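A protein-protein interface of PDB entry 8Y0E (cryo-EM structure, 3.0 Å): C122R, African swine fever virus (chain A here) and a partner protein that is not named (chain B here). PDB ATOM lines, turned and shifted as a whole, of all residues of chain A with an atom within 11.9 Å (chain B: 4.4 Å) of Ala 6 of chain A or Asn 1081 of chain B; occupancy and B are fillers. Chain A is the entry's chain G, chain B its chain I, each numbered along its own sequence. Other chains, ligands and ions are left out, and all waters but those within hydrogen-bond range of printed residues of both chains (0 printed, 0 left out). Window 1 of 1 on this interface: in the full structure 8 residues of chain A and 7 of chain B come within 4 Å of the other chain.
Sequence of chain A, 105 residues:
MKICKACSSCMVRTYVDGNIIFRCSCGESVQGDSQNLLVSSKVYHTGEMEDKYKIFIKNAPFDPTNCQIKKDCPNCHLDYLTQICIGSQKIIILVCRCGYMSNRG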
ATOM      1  N   LYS A   2      16.007  -0.664 -11.975  1.00  0.00           N
ATOM      2  CA  LYS A   2      15.158   0.244 -11.221  1.00  0.00           C
ATOM      3  C   LYS A   2      14.911  -0.345  -9.845  1.00  0.00           C
ATOM      4  O   LYS A   2      14.405  -1.465  -9.728  1.00  0.00           O
ATOM      5  CB  LYS A   2      13.837   0.497 -11.948  1.00  0.00           C
ATOM      6  CG  LYS A   2      13.043   1.647 -11.375  1.00  0.00           C
ATOM      7  CD  LYS A   2      12.491   2.510 -12.486  1.00  0.00           C
ATOM      8  CE  LYS A   2      13.345   3.750 -12.691  1.00  0.00           C
ATOM      9  NZ  LYS A   2      13.231   4.693 -11.548  1.00  0.00           N
ATOM     10  N   ILE A   3      15.269   0.411  -8.812  1.00  0.00           N
ATOM     11  CA  ILE A   3      15.180  -0.040  -7.431  1.00  0.00           C
ATOM     12  C   ILE A   3      14.117   0.773  -6.705  1.00  0.00           C
ATOM     13  O   ILE A   3      13.997   1.987  -6.907  1.00  0.00           O
ATOM     14  CB  ILE A   3      16.548   0.039  -6.722  1.00  0.00           C
ATOM     15  CG1 ILE A   3      17.409   1.179  -7.277  1.00  0.00           C
ATOM     16  CG2 ILE A   3      17.285  -1.281  -6.854  1.00  0.00           C
ATOM     17  CD1 ILE A   3      16.958   2.575  -6.925  1.00  0.00           C
ATOM     18  N   CYS A   4      13.323   0.089  -5.890  1.00  0.00           N
ATOM     19  CA  CYS A   4      12.241   0.744  -5.171  1.00  0.00           C
ATOM     20  C   CYS A   4      12.800   1.785  -4.212  1.00  0.00           C
ATOM     21  O   CYS A   4      13.748   1.517  -3.471  1.00  0.00           O
ATOM     22  CB  CYS A   4      11.414  -0.294  -4.415  1.00  0.00           C
ATOM     23  SG  CYS A   4      10.100   0.390  -3.405  1.00  0.00           S
ATOM     24  N   LYS A   5      12.213   2.981  -4.230  1.00  0.00           N
ATOM     25  CA  LYS A   5      12.659   4.037  -3.332  1.00  0.00           C
ATOM     26  C   LYS A   5      12.372   3.713  -1.873  1.00  0.00           C
ATOM     27  O   LYS A   5      12.944   4.354  -0.986  1.00  0.00           O
ATOM     28  CB  LYS A   5      11.994   5.362  -3.710  1.00  0.00           C
ATOM     29  CG  LYS A   5      12.956   6.529  -3.851  1.00  0.00           C
ATOM     30  CD  LYS A   5      13.953   6.297  -4.968  1.00  0.00           C
ATOM     31  CE  LYS A   5      15.040   7.358  -4.965  1.00  0.00           C
ATOM     32  NZ  LYS A   5      16.146   7.027  -5.904  1.00  0.00           N
ATOM     33  N   ALA A   6      11.501   2.742  -1.605  1.00  0.00           N
ATOM     34  CA  ALA A   6      11.115   2.415  -0.237  1.00  0.00           C
ATOM     35  C   ALA A   6      11.940   1.265   0.332  1.00  0.00           C
ATOM     36  O   ALA A   6      12.679   1.446   1.304  1.00  0.00           O
ATOM     37  CB  ALA A   6       9.624   2.073  -0.185  1.00  0.00           C
ATOM     38  N   CYS A   7      11.836   0.082  -0.269  1.00  0.00           N
ATOM     39  CA  CYS A   7      12.472  -1.110   0.269  1.00  0.00           C
ATOM     40  C   CYS A   7      13.679  -1.556  -0.542  1.00  0.00           C
ATOM     41  O   CYS A   7      14.238  -2.619  -0.260  1.00  0.00           O
ATOM     42  CB  CYS A   7      11.460  -2.251   0.361  1.00  0.00           C
ATOM     43  SG  CYS A   7      10.664  -2.660  -1.200  1.00  0.00           S
ATOM     44  N   SER A   8      14.092  -0.773  -1.535  1.00  0.00           N
ATOM     45  CA  SER A   8      15.262  -1.080  -2.351  1.00  0.00           C
ATOM     46  C   SER A   8      15.181  -2.499  -2.913  1.00  0.00           C
ATOM     47  O   SER A   8      15.947  -3.391  -2.552  1.00  0.00           O
ATOM     48  CB  SER A   8      16.550  -0.872  -1.553  1.00  0.00           C
ATOM     49  OG  SER A   8      16.769   0.504  -1.300  1.00  0.00           O
ATOM     50  N   SER A   9      14.208  -2.698  -3.794  1.00  0.00           N
ATOM     51  CA  SER A   9      14.009  -3.977  -4.453  1.00  0.00           C
ATOM     52  C   SER A   9      13.876  -3.752  -5.950  1.00  0.00           C
ATOM     53  O   SER A   9      13.586  -2.646  -6.408  1.00  0.00           O
ATOM     54  CB  SER A   9      12.773  -4.701  -3.913  1.00  0.00           C
ATOM     55  OG  SER A   9      12.855  -6.093  -4.156  1.00  0.00           O
ATOM     56  N   CYS A  10      14.105  -4.818  -6.713  1.00  0.00           N
ATOM     57  CA  CYS A  10      14.008  -4.728  -8.163  1.00  0.00           C
ATOM     58  C   CYS A  10      12.568  -4.476  -8.588  1.00  0.00           C
ATOM     59  O   CYS A  10      11.626  -5.030  -8.016  1.00  0.00           O
ATOM     60  CB  CYS A  10      14.531  -6.006  -8.815  1.00  0.00           C
ATOM     61  SG  CYS A  10      15.880  -6.800  -7.931  1.00  0.00           S
ATOM     62  N   MET A  11      12.402  -3.641  -9.608  1.00  0.00           N
ATOM     63  CA  MET A  11      11.096  -3.179 -10.055  1.00  0.00           C
ATOM     64  C   MET A  11      10.789  -3.772 -11.424  1.00  0.00           C
ATOM     65  O   MET A  11      11.540  -3.552 -12.379  1.00  0.00           O
ATOM     66  CB  MET A  11      11.070  -1.653 -10.111  1.00  0.00           C
ATOM     67  CG  MET A  11      11.425  -0.989  -8.796  1.00  0.00           C
ATOM     68  SD  MET A  11      10.346   0.395  -8.410  1.00  0.00           S
ATOM     69  CE  MET A  11       8.782  -0.440  -8.226  1.00  0.00           C
ATOM     70  N   PHE A  22       6.421   0.970 -13.079  1.00  0.00           N
ATOM     71  CA  PHE A  22       7.175  -0.081 -12.416  1.00  0.00           C
ATOM     72  C   PHE A  22       6.448  -0.544 -11.165  1.00  0.00           C
ATOM     73  O   PHE A  22       5.936   0.270 -10.394  1.00  0.00           O
ATOM     74  CB  PHE A  22       8.576   0.406 -12.064  1.00  0.00           C
ATOM     75  CG  PHE A  22       9.433   0.673 -13.261  1.00  0.00           C
ATOM     76  CD1 PHE A  22       9.319   1.860 -13.957  1.00  0.00           C
ATOM     77  CD2 PHE A  22      10.346  -0.270 -13.696  1.00  0.00           C
ATOM     78  CE1 PHE A  22      10.103   2.105 -15.060  1.00  0.00           C
ATOM     79  CE2 PHE A  22      11.132  -0.030 -14.800  1.00  0.00           C
ATOM     80  CZ  PHE A  22      11.013   1.159 -15.482  1.00  0.00           C
ATOM     81  N   ARG A  23       6.398  -1.857 -10.973  1.00  0.00           N
ATOM     82  CA  ARG A  23       5.667  -2.456  -9.869  1.00  0.00           C
ATOM     83  C   ARG A  23       6.636  -3.171  -8.940  1.00  0.00           C
ATOM     84  O   ARG A  23       7.428  -4.007  -9.388  1.00  0.00           O
ATOM     85  CB  ARG A  23       4.608  -3.430 -10.384  1.00  0.00           C
ATOM     86  CG  ARG A  23       3.464  -2.756 -11.119  1.00  0.00           C
ATOM     87  CD  ARG A  23       2.273  -2.518 -10.209  1.00  0.00           C
ATOM     88  NE  ARG A  23       2.078  -1.102  -9.925  1.00  0.00           N
ATOM     89  CZ  ARG A  23       1.332  -0.285 -10.658  1.00  0.00           C
ATOM     90  NH1 ARG A  23       0.711  -0.705 -11.747  1.00  0.00           N
ATOM     91  NH2 ARG A  23       1.214   0.988 -10.290  1.00  0.00           N
ATOM     92  N   CYS A  24       6.570  -2.842  -7.657  1.00  0.00           N
ATOM     93  CA  CYS A  24       7.318  -3.542  -6.626  1.00  0.00           C
ATOM     94  C   CYS A  24       6.422  -4.564  -5.940  1.00  0.00           C
ATOM     95  O   CYS A  24       5.202  -4.572  -6.105  1.00  0.00           O
ATOM     96  CB  CYS A  24       7.876  -2.557  -5.598  1.00  0.00           C
ATOM     97  SG  CYS A  24       9.173  -3.242  -4.557  1.00  0.00           S
ATOM     98  N   SER A  25       7.050  -5.447  -5.164  1.00  0.00           N
ATOM     99  CA  SER A  25       6.268  -6.353  -4.332  1.00  0.00           C
ATOM    100  C   SER A  25       5.531  -5.593  -3.236  1.00  0.00           C
ATOM    101  O   SER A  25       4.498  -6.061  -2.744  1.00  0.00           O
ATOM    102  CB  SER A  25       7.169  -7.429  -3.728  1.00  0.00           C
ATOM    103  OG  SER A  25       6.473  -8.193  -2.759  1.00  0.00           O
ATOM    104  N   CYS A  26       6.042  -4.425  -2.849  1.00  0.00           N
ATOM    105  CA  CYS A  26       5.397  -3.585  -1.852  1.00  0.00           C
ATOM    106  C   CYS A  26       4.374  -2.631  -2.453  1.00  0.00           C
ATOM    107  O   CYS A  26       3.655  -1.964  -1.703  1.00  0.00           O
ATOM    108  CB  CYS A  26       6.446  -2.786  -1.078  1.00  0.00           C
ATOM    109  SG  CYS A  26       7.142  -1.396  -1.987  1.00  0.00           S
ATOM    110  N   GLY A  27       4.295  -2.545  -3.779  1.00  0.00           N
ATOM    111  CA  GLY A  27       3.250  -1.802  -4.447  1.00  0.00           C
ATOM    112  C   GLY A  27       3.640  -0.436  -4.967  1.00  0.00           C
ATOM    113  O   GLY A  27       2.861   0.158  -5.720  1.00  0.00           O
ATOM    114  N   GLU A  28       4.809   0.081  -4.602  1.00  0.00           N
ATOM    115  CA  GLU A  28       5.183   1.419  -5.037  1.00  0.00           C
ATOM    116  C   GLU A  28       5.439   1.440  -6.538  1.00  0.00           C
ATOM    117  O   GLU A  28       5.903   0.457  -7.118  1.00  0.00           O
ATOM    118  CB  GLU A  28       6.420   1.900  -4.282  1.00  0.00           C
ATOM    119  CG  GLU A  28       6.725   3.374  -4.490  1.00  0.00           C
ATOM    120  CD  GLU A  28       8.195   3.652  -4.724  1.00  0.00           C
ATOM    121  OE1 GLU A  28       8.529   4.270  -5.755  1.00  0.00           O
ATOM    122  OE2 GLU A  28       9.017   3.266  -3.872  1.00  0.00           O
ATOM    123  N   SER A  29       5.117   2.568  -7.172  1.00  0.00           N
ATOM    124  CA  SER A  29       5.344   2.765  -8.597  1.00  0.00           C
ATOM    125  C   SER A  29       6.037   4.102  -8.821  1.00  0.00           C
ATOM    126  O   SER A  29       5.842   5.052  -8.059  1.00  0.00           O
ATOM    127  CB  SER A  29       4.033   2.700  -9.384  1.00  0.00           C
ATOM    128  OG  SER A  29       3.462   1.407  -9.293  1.00  0.00           O
ATOM    129  N   VAL A  30       6.852   4.172  -9.874  1.00  0.00           N
ATOM    130  CA  VAL A  30       7.810   5.258 -10.038  1.00  0.00           C
ATOM    131  C   VAL A  30       7.614   6.055 -11.319  1.00  0.00           C
ATOM    132  O   VAL A  30       8.261   7.093 -11.481  1.00  0.00           O
ATOM    133  CB  VAL A  30       9.259   4.740  -9.964  1.00  0.00           C
ATOM    134  CG1 VAL A  30       9.412   3.742  -8.836  1.00  0.00           C
ATOM    135  CG2 VAL A  30       9.643   4.116 -11.278  1.00  0.00           C
ATOM    136  N   LEU B1077       9.780  -0.693   6.686  1.00  0.00           N
ATOM    137  CA  LEU B1077       9.339   0.152   5.583  1.00  0.00           C
ATOM    138  C   LEU B1077       8.597  -0.646   4.522  1.00  0.00           C
ATOM    139  O   LEU B1077       7.647  -0.138   3.920  1.00  0.00           O
ATOM    140  CB  LEU B1077      10.534   0.878   4.975  1.00  0.00           C
ATOM    141  CG  LEU B1077      11.219   1.827   5.955  1.00  0.00           C
ATOM    142  CD1 LEU B1077      12.302   2.642   5.272  1.00  0.00           C
ATOM    143  CD2 LEU B1077      10.191   2.732   6.597  1.00  0.00           C
ATOM    144  N   TYR B1078       9.001  -1.892   4.282  1.00  0.00           N
ATOM    145  CA  TYR B1078       8.304  -2.728   3.315  1.00  0.00           C
ATOM    146  C   TYR B1078       6.884  -3.019   3.773  1.00  0.00           C
ATOM    147  O   TYR B1078       5.933  -2.898   2.995  1.00  0.00           O
ATOM    148  CB  TYR B1078       9.083  -4.024   3.099  1.00  0.00           C
ATOM    149  CG  TYR B1078       8.370  -5.061   2.264  1.00  0.00           C
ATOM    150  CD1 TYR B1078       8.320  -4.951   0.883  1.00  0.00           C
ATOM    151  CD2 TYR B1078       7.771  -6.164   2.855  1.00  0.00           C
ATOM    152  CE1 TYR B1078       7.681  -5.900   0.118  1.00  0.00           C
ATOM    153  CE2 TYR B1078       7.131  -7.120   2.096  1.00  0.00           C
ATOM    154  CZ  TYR B1078       7.087  -6.983   0.728  1.00  0.00           C
ATOM    155  OH  TYR B1078       6.449  -7.932  -0.036  1.00  0.00           O
ATOM    156  N   ASN B1079       6.719  -3.395   5.044  1.00  0.00           N
ATOM    157  CA  ASN B1079       5.379  -3.648   5.564  1.00  0.00           C
ATOM    158  C   ASN B1079       4.529  -2.386   5.526  1.00  0.00           C
ATOM    159  O   ASN B1079       3.344  -2.432   5.169  1.00  0.00           O
ATOM    160  CB  ASN B1079       5.468  -4.194   6.983  1.00  0.00           C
ATOM    161  CG  ASN B1079       6.345  -5.414   7.074  1.00  0.00           C
ATOM    162  OD1 ASN B1079       6.512  -6.144   6.099  1.00  0.00           O
ATOM    163  ND2 ASN B1079       6.920  -5.644   8.246  1.00  0.00           N
ATOM    164  N   TYR B1080       5.120  -1.245   5.883  1.00  0.00           N
ATOM    165  CA  TYR B1080       4.386   0.009   5.806  1.00  0.00           C
ATOM    166  C   TYR B1080       3.983   0.341   4.377  1.00  0.00           C
ATOM    167  O   TYR B1080       2.911   0.907   4.153  1.00  0.00           O
ATOM    168  CB  TYR B1080       5.219   1.143   6.389  1.00  0.00           C
ATOM    169  CG  TYR B1080       4.542   2.478   6.280  1.00  0.00           C
ATOM    170  CD1 TYR B1080       3.243   2.654   6.726  1.00  0.00           C
ATOM    171  CD2 TYR B1080       5.199   3.562   5.722  1.00  0.00           C
ATOM    172  CE1 TYR B1080       2.618   3.869   6.622  1.00  0.00           C
ATOM    173  CE2 TYR B1080       4.585   4.783   5.615  1.00  0.00           C
ATOM    174  CZ  TYR B1080       3.293   4.931   6.065  1.00  0.00           C
ATOM    175  OH  TYR B1080       2.677   6.156   5.957  1.00  0.00           O
ATOM    176  N   ASN B1081       4.827   0.009   3.400  1.00  0.00           N
ATOM    177  CA  ASN B1081       4.469   0.275   2.013  1.00  0.00           C
ATOM    178  C   ASN B1081       3.376  -0.662   1.519  1.00  0.00           C
ATOM    179  O   ASN B1081       2.539  -0.250   0.709  1.00  0.00           O
ATOM    180  CB  ASN B1081       5.700   0.177   1.119  1.00  0.00           C
ATOM    181  CG  ASN B1081       5.835   1.366   0.199  1.00  0.00           C
ATOM    182  OD1 ASN B1081       5.366   2.459   0.510  1.00  0.00           O
ATOM    183  ND2 ASN B1081       6.472   1.159  -0.946  1.00  0.00           N
ATOM    184  N   CYS B1082       3.365  -1.919   1.971  1.00  0.00           N
ATOM    185  CA  CYS B1082       2.210  -2.764   1.674  1.00  0.00           C
ATOM    186  C   CYS B1082       0.944  -2.174   2.276  1.00  0.00           C
ATOM    187  O   CYS B1082      -0.117  -2.190   1.644  1.00  0.00           O
ATOM    188  CB  CYS B1082       2.397  -4.201   2.169  1.00  0.00           C
ATOM    189  SG  CYS B1082       4.051  -4.894   2.183  1.00  0.00           S
ATOM    190  N   LEU B1083       1.036  -1.650   3.500  1.00  0.00           N
ATOM    191  CA  LEU B1083      -0.128  -1.023   4.118  1.00  0.00           C
ATOM    192  C   LEU B1083      -0.587   0.200   3.333  1.00  0.00           C
ATOM    193  O   LEU B1083      -1.792   0.423   3.168  1.00  0.00           O
ATOM    194  CB  LEU B1083       0.183  -0.639   5.563  1.00  0.00           C
ATOM    195  CG  LEU B1083      -0.929   0.121   6.287  1.00  0.00           C
ATOM    196  CD1 LEU B1083      -2.119  -0.785   6.536  1.00  0.00           C
ATOM    197  CD2 LEU B1083      -0.416   0.707   7.587  1.00  0.00           C
ATOM    198  N   ARG B1084       0.357   1.007   2.849  1.00  0.00           N
ATOM    199  CA  ARG B1084      -0.003   2.234   2.147  1.00  0.00           C
ATOM    200  C   ARG B1084      -0.764   1.940   0.861  1.00  0.00           C
ATOM    201  O   ARG B1084      -1.742   2.624   0.540  1.00  0.00           O
ATOM    202  CB  ARG B1084       1.250   3.050   1.840  1.00  0.00           C
ATOM    203  CG  ARG B1084       1.724   3.927   2.978  1.00  0.00           C
ATOM    204  CD  ARG B1084       1.835   5.374   2.535  1.00  0.00           C
ATOM    205  NE  ARG B1084       2.440   5.502   1.217  1.00  0.00           N
ATOM    206  CZ  ARG B1084       3.741   5.418   0.977  1.00  0.00           C
ATOM    207  NH1 ARG B1084       4.611   5.208   1.951  1.00  0.00           N
ATOM    208  NH2 ARG B1084       4.182   5.548  -0.270  1.00  0.00           N
ATOM    209  N   HIS B1085      -0.336   0.928   0.116  1.00  0.00           N
ATOM    210  CA  HIS B1085      -0.871   0.637  -1.209  1.00  0.00           C
ATOM    211  C   HIS B1085      -1.709  -0.637  -1.219  1.00  0.00           C
ATOM    212  O   HIS B1085      -1.629  -1.438  -2.149  1.00  0.00           O
ATOM    213  CB  HIS B1085       0.256   0.530  -2.230  1.00  0.00           C
ATOM    214  CG  HIS B1085       1.125   1.745  -2.304  1.00  0.00           C
ATOM    215  ND1 HIS B1085       2.270   1.887  -1.551  1.00  0.00           N
ATOM    216  CD2 HIS B1085       1.022   2.872  -3.048  1.00  0.00           C
ATOM    217  CE1 HIS B1085       2.831   3.051  -1.823  1.00  0.00           C
ATOM    218  NE2 HIS B1085       2.095   3.668  -2.729  1.00  0.00           N
ATOM    219  N   VAL B1119       9.449   6.913   4.598  1.00  0.00           N
ATOM    220  CA  VAL B1119      10.741   6.367   4.192  1.00  0.00           C
ATOM    221  C   VAL B1119      11.809   7.451   4.214  1.00  0.00           C
ATOM    222  O   VAL B1119      12.970   7.191   4.550  1.00  0.00           O
ATOM    223  CB  VAL B1119      10.630   5.706   2.807  1.00  0.00           C
ATOM    224  CG1 VAL B1119      11.917   4.980   2.465  1.00  0.00           C
ATOM    225  CG2 VAL B1119       9.452   4.750   2.776  1.00  0.00           C
ATOM    226  N   HIS B1123      17.662   5.607   3.008  1.00  0.00           N
ATOM    227  CA  HIS B1123      18.591   4.698   2.346  1.00  0.00           C
ATOM    228  C   HIS B1123      19.895   5.398   1.990  1.00  0.00           C
ATOM    229  O   HIS B1123      20.986   4.903   2.300  1.00  0.00           O
ATOM    230  CB  HIS B1123      17.938   4.107   1.099  1.00  0.00           C
ATOM    231  CG  HIS B1123      16.752   3.243   1.391  1.00  0.00           C
ATOM    232  ND1 HIS B1123      16.859   1.894   1.645  1.00  0.00           N
ATOM    233  CD2 HIS B1123      15.433   3.535   1.466  1.00  0.00           C
ATOM    234  CE1 HIS B1123      15.658   1.392   1.866  1.00  0.00           C
ATOM    235  NE2 HIS B1123      14.774   2.368   1.762  1.00  0.00           N
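A ring nitrogen (ND1) of His 1123 of chain B lies within hydrogen-bond range of the side-chain hydroxyl (OG) of Ser 8 of chain A (3.3 Å).
The side-chain hydroxyl of Tyr 1078 of chain B lies within hydrogen-bond range of the side-chain hydroxyl of Ser 25 of chain A (2.7 Å).
ND2 of Asn 1081 of chain B sits close to SG of Cys 26 of chain A.
A ring nitrogen (NE2) of His 1123 of chain B lies close to the backbone carbonyl oxygen (O) of Ala 6 of chain A, at 2.3 Å.
N of Ala 6 of chain A lies close to SG of Cys 4 of chain A, 3.3 Å away.
The side-chain sulfur (SG) of Cys 4 of chain A lies close to the side-chain carboxylate (OE2) of Glu 28 of chain A (3.1 Å).
The side-chain carboxylate (OE2) of Glu 28 of chain A lies within hydrogen-bond range of the backbone NH (N) of Lys 5 of chain A (3.2 Å).
N of Ala 6 of chain A is in hydrogen-bond range of OE2 of Glu 28 of chain A, at 3.4 Å.
O of Tyr 1078 of chain B lies within hydrogen-bond range of SG of Cys 1082 of chain B, at 2.9 Å.
The backbone carbonyl oxygen of Asn 1081 of chain B sits at hydrogen-bond distance from a ring nitrogen (ND1) of His 1085 of chain B, at 3.1 Å.
Among the printed residues, pairs that only touch across the chains: Lys 5 of chain A with Val 1119 of chain B (3.7 Å), Lys 5 of chain A with His 1123 of chain B (3.6 Å), Ala 6 of chain A with Asn 1081 of chain B (3.4 Å), Ala 6 of chain A with Val 1119 of chain B (3.8 Å), Cys 7 of chain A with Tyr 1078 of chain B (3.9 Å), Cys 26 of chain A with Tyr 1078 of chain B (3.5 Å), Cys 26 of chain A with Cys 1082 of chain B (3.7 Å) and Glu 28 of chain A with Asn 1081 of chain B (3.4 Å).
Ala 6 of chain A touches just these residues of chain B: Asn 1081, Val 1119 and His 1123.
Of the printed residues of chain A, Asn 1081 of chain B touches Ala 6 (3.4 Å), Cys 26 (2.8 Å) and Glu 28 (3.4 Å).
No residue of chain A comes within 4 Å of Leu 1077 of chain B.
No residue of chain A comes within 4 Å of Asn 1079 of chain B.
No residue of chain A comes within 4 Å of Tyr 1080 of chain B.
Cys 1082 of chain B touches just one residue of chain A: Cys 26.
No residue of chain A comes within 4 Å of Leu 1083 of chain B.
Arg 1084 of chain B touches none of the printed residues of chain A.
No residue of chain A comes within 4 Å of His 1085 of chain B.
Of the printed residues of chain B, Lys 5 of chain A touches Val 1119 and His 1123.
Of the printed residues of chain B, Cys 7 of chain A touches Tyr 1078 (3.9 Å).
The nearest residue of chain B that does not touch Ala 6 of chain A is Leu 1077 of chain B (4.2 Å).
The nearest residue of chain A that does not touch Asn 1081 of chain B is Cys 4 of chain A (4.4 Å).
Hydrophobic or aromatic side chains of chain B that line the printed part of chain A: Tyr 1078, Val 1119 and His 1123.
Along chain A the printed residues that touch a printed residue of chain B span positions 5 to 28.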
